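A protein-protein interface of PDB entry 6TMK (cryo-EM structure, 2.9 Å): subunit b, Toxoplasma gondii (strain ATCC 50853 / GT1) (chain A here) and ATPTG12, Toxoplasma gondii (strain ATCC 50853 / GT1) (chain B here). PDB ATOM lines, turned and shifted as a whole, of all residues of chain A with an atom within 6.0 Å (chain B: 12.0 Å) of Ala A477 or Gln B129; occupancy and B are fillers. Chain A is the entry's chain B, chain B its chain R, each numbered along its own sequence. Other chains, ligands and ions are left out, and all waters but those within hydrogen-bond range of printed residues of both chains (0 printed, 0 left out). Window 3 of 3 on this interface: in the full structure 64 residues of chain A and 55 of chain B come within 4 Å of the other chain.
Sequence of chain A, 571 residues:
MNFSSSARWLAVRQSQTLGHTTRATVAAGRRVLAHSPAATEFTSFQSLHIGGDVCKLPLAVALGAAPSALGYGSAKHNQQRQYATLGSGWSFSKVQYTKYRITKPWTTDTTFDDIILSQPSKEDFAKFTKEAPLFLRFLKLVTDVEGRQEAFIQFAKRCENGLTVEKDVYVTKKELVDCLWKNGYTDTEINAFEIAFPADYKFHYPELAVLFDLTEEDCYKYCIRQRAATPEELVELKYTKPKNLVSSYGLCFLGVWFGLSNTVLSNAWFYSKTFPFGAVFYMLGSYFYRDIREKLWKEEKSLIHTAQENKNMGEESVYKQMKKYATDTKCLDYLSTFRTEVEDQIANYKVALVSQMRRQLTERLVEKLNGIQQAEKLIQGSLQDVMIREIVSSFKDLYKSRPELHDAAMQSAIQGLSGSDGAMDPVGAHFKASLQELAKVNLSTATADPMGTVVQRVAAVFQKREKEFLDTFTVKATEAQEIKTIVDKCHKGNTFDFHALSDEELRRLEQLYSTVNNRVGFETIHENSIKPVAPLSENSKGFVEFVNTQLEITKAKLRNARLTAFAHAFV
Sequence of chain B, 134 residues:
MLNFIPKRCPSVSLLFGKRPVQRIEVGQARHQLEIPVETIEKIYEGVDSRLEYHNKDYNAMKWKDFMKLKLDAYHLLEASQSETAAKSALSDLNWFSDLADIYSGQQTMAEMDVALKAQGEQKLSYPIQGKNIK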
ATOM      1  N   LYS A 467      17.075   2.999  15.459  1.00  0.00           N
ATOM      2  CA  LYS A 467      16.313   1.903  14.871  1.00  0.00           C
ATOM      3  C   LYS A 467      17.051   0.579  15.025  1.00  0.00           C
ATOM      4  O   LYS A 467      16.446  -0.438  15.387  1.00  0.00           O
ATOM      5  CB  LYS A 467      16.031   2.191  13.397  1.00  0.00           C
ATOM      6  CG  LYS A 467      15.103   3.374  13.168  1.00  0.00           C
ATOM      7  CD  LYS A 467      13.653   2.993  13.414  1.00  0.00           C
ATOM      8  CE  LYS A 467      12.712   4.145  13.099  1.00  0.00           C
ATOM      9  NZ  LYS A 467      11.309   3.687  12.907  1.00  0.00           N
ATOM     10  N   PHE A 469      18.927  -0.084  17.326  1.00  0.00           N
ATOM     11  CA  PHE A 469      18.849  -0.381  18.751  1.00  0.00           C
ATOM     12  C   PHE A 469      17.511  -1.030  19.083  1.00  0.00           C
ATOM     13  O   PHE A 469      17.462  -2.085  19.733  1.00  0.00           O
ATOM     14  CB  PHE A 469      19.054   0.910  19.548  1.00  0.00           C
ATOM     15  CG  PHE A 469      18.603   0.831  20.978  1.00  0.00           C
ATOM     16  CD1 PHE A 469      19.484   0.450  21.974  1.00  0.00           C
ATOM     17  CD2 PHE A 469      17.310   1.178  21.328  1.00  0.00           C
ATOM     18  CE1 PHE A 469      19.076   0.394  23.291  1.00  0.00           C
ATOM     19  CE2 PHE A 469      16.895   1.119  22.643  1.00  0.00           C
ATOM     20  CZ  PHE A 469      17.778   0.724  23.625  1.00  0.00           C
ATOM     21  N   LEU A 470      16.416  -0.368  18.703  1.00  0.00           N
ATOM     22  CA  LEU A 470      15.098  -0.861  19.079  1.00  0.00           C
ATOM     23  C   LEU A 470      14.799  -2.187  18.395  1.00  0.00           C
ATOM     24  O   LEU A 470      14.044  -3.000  18.936  1.00  0.00           O
ATOM     25  CB  LEU A 470      14.028   0.170  18.720  1.00  0.00           C
ATOM     26  CG  LEU A 470      13.810   1.353  19.670  1.00  0.00           C
ATOM     27  CD1 LEU A 470      12.604   2.160  19.218  1.00  0.00           C
ATOM     28  CD2 LEU A 470      13.632   0.901  21.112  1.00  0.00           C
ATOM     29  N   ASP A 471      15.396  -2.440  17.225  1.00  0.00           N
ATOM     30  CA  ASP A 471      15.174  -3.712  16.553  1.00  0.00           C
ATOM     31  C   ASP A 471      15.884  -4.858  17.255  1.00  0.00           C
ATOM     32  O   ASP A 471      15.608  -6.023  16.949  1.00  0.00           O
ATOM     33  CB  ASP A 471      15.640  -3.628  15.099  1.00  0.00           C
ATOM     34  CG  ASP A 471      15.187  -4.816  14.274  1.00  0.00           C
ATOM     35  OD1 ASP A 471      15.931  -5.223  13.356  1.00  0.00           O
ATOM     36  OD2 ASP A 471      14.095  -5.353  14.554  1.00  0.00           O
ATOM     37  N   THR A 472      16.785  -4.547  18.188  1.00  0.00           N
ATOM     38  CA  THR A 472      17.588  -5.540  18.880  1.00  0.00           C
ATOM     39  C   THR A 472      17.195  -5.692  20.338  1.00  0.00           C
ATOM     40  O   THR A 472      17.451  -6.750  20.923  1.00  0.00           O
ATOM     41  CB  THR A 472      19.079  -5.174  18.804  1.00  0.00           C
ATOM     42  OG1 THR A 472      19.241  -3.768  19.023  1.00  0.00           O
ATOM     43  CG2 THR A 472      19.650  -5.543  17.445  1.00  0.00           C
ATOM     44  N   THR A 474      13.837  -4.810  21.168  1.00  0.00           N
ATOM     45  CA  THR A 474      12.382  -4.816  21.131  1.00  0.00           C
ATOM     46  C   THR A 474      11.934  -5.705  19.981  1.00  0.00           C
ATOM     47  O   THR A 474      12.717  -6.036  19.088  1.00  0.00           O
ATOM     48  CB  THR A 474      11.812  -3.399  20.977  1.00  0.00           C
ATOM     49  OG1 THR A 474      12.547  -2.491  21.806  1.00  0.00           O
ATOM     50  CG2 THR A 474      10.343  -3.367  21.380  1.00  0.00           C
ATOM     51  N   VAL A 475      10.660  -6.085  20.016  1.00  0.00           N
ATOM     52  CA  VAL A 475      10.072  -6.872  18.939  1.00  0.00           C
ATOM     53  C   VAL A 475       9.614  -5.929  17.836  1.00  0.00           C
ATOM     54  O   VAL A 475       9.318  -4.753  18.077  1.00  0.00           O
ATOM     55  CB  VAL A 475       8.906  -7.733  19.463  1.00  0.00           C
ATOM     56  CG1 VAL A 475       7.700  -6.861  19.775  1.00  0.00           C
ATOM     57  CG2 VAL A 475       8.547  -8.810  18.454  1.00  0.00           C
ATOM     58  N   LYS A 476       9.554  -6.446  16.612  1.00  0.00           N
ATOM     59  CA  LYS A 476       9.158  -5.643  15.466  1.00  0.00           C
ATOM     60  C   LYS A 476       7.667  -5.777  15.183  1.00  0.00           C
ATOM     61  O   LYS A 476       7.070  -6.849  15.358  1.00  0.00           O
ATOM     62  CB  LYS A 476       9.959  -6.044  14.227  1.00  0.00           C
ATOM     63  CG  LYS A 476       9.898  -5.014  13.111  1.00  0.00           C
ATOM     64  CD  LYS A 476      10.808  -5.380  11.949  1.00  0.00           C
ATOM     65  CE  LYS A 476      12.271  -5.165  12.295  1.00  0.00           C
ATOM     66  NZ  LYS A 476      13.010  -4.470  11.204  1.00  0.00           N
ATOM     67  N   ALA A 477       7.072  -4.670  14.736  1.00  0.00           N
ATOM     68  CA  ALA A 477       5.635  -4.646  14.511  1.00  0.00           C
ATOM     69  C   ALA A 477       5.233  -5.576  13.378  1.00  0.00           C
ATOM     70  O   ALA A 477       4.105  -6.072  13.364  1.00  0.00           O
ATOM     71  CB  ALA A 477       5.172  -3.221  14.213  1.00  0.00           C
ATOM     72  N   THR A 478       6.134  -5.837  12.426  1.00  0.00           N
ATOM     73  CA  THR A 478       5.824  -6.816  11.390  1.00  0.00           C
ATOM     74  C   THR A 478       5.735  -8.220  11.977  1.00  0.00           C
ATOM     75  O   THR A 478       4.809  -8.976  11.656  1.00  0.00           O
ATOM     76  CB  THR A 478       6.871  -6.759  10.274  1.00  0.00           C
ATOM     77  OG1 THR A 478       6.462  -7.603   9.189  1.00  0.00           O
ATOM     78  CG2 THR A 478       8.237  -7.215  10.775  1.00  0.00           C
ATOM     79  N   GLU A 479       6.687  -8.585  12.840  1.00  0.00           N
ATOM     80  CA  GLU A 479       6.619  -9.873  13.520  1.00  0.00           C
ATOM     81  C   GLU A 479       5.339  -9.991  14.335  1.00  0.00           C
ATOM     82  O   GLU A 479       4.691 -11.044  14.339  1.00  0.00           O
ATOM     83  CB  GLU A 479       7.846 -10.057  14.411  1.00  0.00           C
ATOM     84  CG  GLU A 479       9.161 -10.086  13.650  1.00  0.00           C
ATOM     85  CD  GLU A 479      10.213 -10.936  14.334  1.00  0.00           C
ATOM     86  OE1 GLU A 479      10.179 -11.042  15.578  1.00  0.00           O
ATOM     87  OE2 GLU A 479      11.074 -11.503  13.627  1.00  0.00           O
ATOM     88  N   ALA A 480       4.961  -8.919  15.033  1.00  0.00           N
ATOM     89  CA  ALA A 480       3.691  -8.920  15.753  1.00  0.00           C
ATOM     90  C   ALA A 480       2.530  -9.162  14.794  1.00  0.00           C
ATOM     91  O   ALA A 480       1.837 -10.185  14.873  1.00  0.00           O
ATOM     92  CB  ALA A 480       3.512  -7.598  16.500  1.00  0.00           C
ATOM     93  N   GLN A 481       2.340  -8.236  13.850  1.00  0.00           N
ATOM     94  CA  GLN A 481       1.224  -8.271  12.912  1.00  0.00           C
ATOM     95  C   GLN A 481       1.068  -9.640  12.265  1.00  0.00           C
ATOM     96  O   GLN A 481      -0.046 -10.165  12.163  1.00  0.00           O
ATOM     97  CB  GLN A 481       1.425  -7.198  11.840  1.00  0.00           C
ATOM     98  CG  GLN A 481       0.852  -5.840  12.201  1.00  0.00           C
ATOM     99  CD  GLN A 481       1.047  -4.816  11.101  1.00  0.00           C
ATOM    100  OE1 GLN A 481       1.703  -5.087  10.095  1.00  0.00           O
ATOM    101  NE2 GLN A 481       0.480  -3.631  11.289  1.00  0.00           N
ATOM    102  N   GLU A 482       2.176 -10.234  11.814  1.00  0.00           N
ATOM    103  CA  GLU A 482       2.102 -11.535  11.159  1.00  0.00           C
ATOM    104  C   GLU A 482       1.253 -12.506  11.969  1.00  0.00           C
ATOM    105  O   GLU A 482       0.222 -12.994  11.494  1.00  0.00           O
ATOM    106  CB  GLU A 482       3.511 -12.094  10.954  1.00  0.00           C
ATOM    107  CG  GLU A 482       4.262 -11.471   9.790  1.00  0.00           C
ATOM    108  CD  GLU A 482       3.777 -11.979   8.447  1.00  0.00           C
ATOM    109  OE1 GLU A 482       3.357 -13.152   8.366  1.00  0.00           O
ATOM    110  OE2 GLU A 482       3.813 -11.203   7.469  1.00  0.00           O
ATOM    111  N   SER B 125       2.929  -7.629  29.175  1.00  0.00           N
ATOM    112  CA  SER B 125       3.068  -6.286  28.610  1.00  0.00           C
ATOM    113  C   SER B 125       4.276  -6.333  27.679  1.00  0.00           C
ATOM    114  O   SER B 125       5.413  -6.132  28.113  1.00  0.00           O
ATOM    115  CB  SER B 125       3.230  -5.235  29.705  1.00  0.00           C
ATOM    116  OG  SER B 125       4.139  -5.672  30.702  1.00  0.00           O
ATOM    117  N   TYR B 126       4.026  -6.597  26.400  1.00  0.00           N
ATOM    118  CA  TYR B 126       5.120  -6.660  25.438  1.00  0.00           C
ATOM    119  C   TYR B 126       5.313  -5.297  24.782  1.00  0.00           C
ATOM    120  O   TYR B 126       4.355  -4.746  24.228  1.00  0.00           O
ATOM    121  CB  TYR B 126       4.824  -7.698  24.365  1.00  0.00           C
ATOM    122  CG  TYR B 126       5.190  -9.111  24.755  1.00  0.00           C
ATOM    123  CD1 TYR B 126       6.505  -9.552  24.704  1.00  0.00           C
ATOM    124  CD2 TYR B 126       4.214 -10.006  25.168  1.00  0.00           C
ATOM    125  CE1 TYR B 126       6.837 -10.847  25.060  1.00  0.00           C
ATOM    126  CE2 TYR B 126       4.534 -11.300  25.523  1.00  0.00           C
ATOM    127  CZ  TYR B 126       5.845 -11.716  25.469  1.00  0.00           C
ATOM    128  OH  TYR B 126       6.161 -13.005  25.823  1.00  0.00           O
ATOM    129  N   PRO B 127       6.517  -4.721  24.816  1.00  0.00           N
ATOM    130  CA  PRO B 127       6.762  -3.491  24.051  1.00  0.00           C
ATOM    131  C   PRO B 127       6.898  -3.794  22.566  1.00  0.00           C
ATOM    132  O   PRO B 127       7.698  -4.643  22.165  1.00  0.00           O
ATOM    133  CB  PRO B 127       8.076  -2.962  24.641  1.00  0.00           C
ATOM    134  CG  PRO B 127       8.775  -4.182  25.114  1.00  0.00           C
ATOM    135  CD  PRO B 127       7.693  -5.104  25.618  1.00  0.00           C
ATOM    136  N   ILE B 128       6.114  -3.095  21.750  1.00  0.00           N
ATOM    137  CA  ILE B 128       6.046  -3.345  20.316  1.00  0.00           C
ATOM    138  C   ILE B 128       6.341  -2.042  19.591  1.00  0.00           C
ATOM    139  O   ILE B 128       5.829  -0.981  19.966  1.00  0.00           O
ATOM    140  CB  ILE B 128       4.669  -3.903  19.896  1.00  0.00           C
ATOM    141  CG1 ILE B 128       3.548  -3.152  20.616  1.00  0.00           C
ATOM    142  CG2 ILE B 128       4.591  -5.395  20.187  1.00  0.00           C
ATOM    143  CD1 ILE B 128       2.177  -3.385  20.019  1.00  0.00           C
ATOM    144  N   GLN B 129       7.170  -2.122  18.552  1.00  0.00           N
ATOM    145  CA  GLN B 129       7.556  -0.923  17.824  1.00  0.00           C
ATOM    146  C   GLN B 129       6.337  -0.264  17.193  1.00  0.00           C
ATOM    147  O   GLN B 129       5.445  -0.937  16.669  1.00  0.00           O
ATOM    148  CB  GLN B 129       8.583  -1.270  16.747  1.00  0.00           C
ATOM    149  CG  GLN B 129       9.979  -1.518  17.287  1.00  0.00           C
ATOM    150  CD  GLN B 129      11.004  -1.708  16.188  1.00  0.00           C
ATOM    151  OE1 GLN B 129      10.681  -1.640  15.002  1.00  0.00           O
ATOM    152  NE2 GLN B 129      12.250  -1.952  16.577  1.00  0.00           N
ATOM    153  N   GLY B 130       6.299   1.066  17.251  1.00  0.00           N
ATOM    154  CA  GLY B 130       5.237   1.843  16.661  1.00  0.00           C
ATOM    155  C   GLY B 130       4.057   2.110  17.575  1.00  0.00           C
ATOM    156  O   GLY B 130       3.390   3.139  17.422  1.00  0.00           O
ATOM    157  N   LYS B 131       3.785   1.214  18.524  1.00  0.00           N
ATOM    158  CA  LYS B 131       2.625   1.333  19.398  1.00  0.00           C
ATOM    159  C   LYS B 131       3.018   1.594  20.845  1.00  0.00           C
ATOM    160  O   LYS B 131       2.637   2.619  21.417  1.00  0.00           O
ATOM    161  CB  LYS B 131       1.775   0.059  19.302  1.00  0.00           C
ATOM    162  CG  LYS B 131       1.187  -0.200  17.923  1.00  0.00           C
ATOM    163  CD  LYS B 131       0.183   0.868  17.524  1.00  0.00           C
ATOM    164  CE  LYS B 131      -0.756   0.363  16.439  1.00  0.00           C
ATOM    165  NZ  LYS B 131      -1.408   1.476  15.695  1.00  0.00           N
ATOM    166  N   ASN B 132       3.779   0.686  21.460  1.00  0.00           N
ATOM    167  CA  ASN B 132       4.132   0.828  22.866  1.00  0.00           C
ATOM    168  C   ASN B 132       5.265   1.818  23.093  1.00  0.00           C
ATOM    169  O   ASN B 132       5.424   2.309  24.217  1.00  0.00           O
ATOM    170  CB  ASN B 132       4.520  -0.532  23.448  1.00  0.00           C
ATOM    171  CG  ASN B 132       4.077  -0.697  24.888  1.00  0.00           C
ATOM    172  OD1 ASN B 132       4.117   0.249  25.674  1.00  0.00           O
ATOM    173  ND2 ASN B 132       3.652  -1.904  25.241  1.00  0.00           N
ATOM    174  N   ILE B 133       6.049   2.120  22.064  1.00  0.00           N
ATOM    175  CA  ILE B 133       7.180   3.027  22.205  1.00  0.00           C
ATOM    176  C   ILE B 133       6.752   4.446  21.851  1.00  0.00           C
ATOM    177  O   ILE B 133       6.528   4.764  20.683  1.00  0.00           O
ATOM    178  CB  ILE B 133       8.361   2.570  21.334  1.00  0.00           C
ATOM    179  CG1 ILE B 133       8.957   1.277  21.892  1.00  0.00           C
ATOM    180  CG2 ILE B 133       9.427   3.652  21.268  1.00  0.00           C
ATOM    181  CD1 ILE B 133       9.547   0.374  20.836  1.00  0.00           C
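N of Gln B129 lies close to O of Val A475 (3.4 Å).
The backbone NH of Asp A471 sits close to the side-chain amide nitrogen of Gln B129, at 3.2 Å.
The backbone carbonyl oxygen of Leu A470 lies close to the side-chain amide nitrogen of Gln B129 (3.1 Å).
The side-chain carboxylate (OD2) of Asp A471 lies within salt-bridge range of the side-chain amino group (NZ) of Lys A476, at 3.6 Å.
O of Leu A470 sits close to OG1 of Thr A474 (3.3 Å).
Among the printed residues, pairs that only touch across the chains: Thr A474 with Pro B127, Val A475 with Pro B127, Ala A477 with Gln B129, Val A475 with Ile B128, Thr A474 with Ile B133, Leu A470 with Ile B133 and Lys A476 with Gln B129.
Gln B129 touches just these residues of chain A: Leu A470 (3.1 Å), Asp A471 (3.2 Å), Val A475 (3.4 Å), Lys A476 (3.9 Å) and Ala A477 (3.4 Å).
Leu A470 touches just these residues of chain B: Gln B129 and Ile B133.
Of chain B, only Gln B129 (3.2 Å) comes within 4 Å of Asp A471.
Of the printed residues of chain B, Thr A474 touches Pro B127 (3.0 Å) and Ile B133 (3.9 Å).
Of chain B, only Pro B127 (3.3 Å), Ile B128 (3.5 Å) and Gln B129 (3.4 Å) come within 4 Å of Val A475.
Of chain B, only Gln B129 comes within 4 Å of Lys A476.
No residue of chain B comes within 4 Å of Thr A478.
Ala A480 touches none of the printed residues of chain B.
No residue of chain B comes within 4 Å of Gln A481.
Of the printed residues of chain A, Ile B133 touches Leu A470 and Thr A474.
Of the printed residues of chain A, Ile B128 touches Val A475 (3.5 Å).
Printed residues of chain A within 4 Å of Pro B127: Thr A474 and Val A475.
Ser B125 touches none of the printed residues of chain A.
Phe A469 touches none of the printed residues of chain B.
The nearest residue of chain B that does not touch Ala A477 is Gly B130 (5.4 Å).
The nearest residue of chain A that does not touch Gln B129 is Thr A474 (4.4 Å).
The nearest printed residue of chain A that does not touch Pro B127 is Lys A476 (6.1 Å).
Printed residues of chain B that touch a printed residue of chain A: Pro B127, Ile B128, Gln B129 and Ile B133.
Among the printed residues, 10 pairs touch across the chains.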
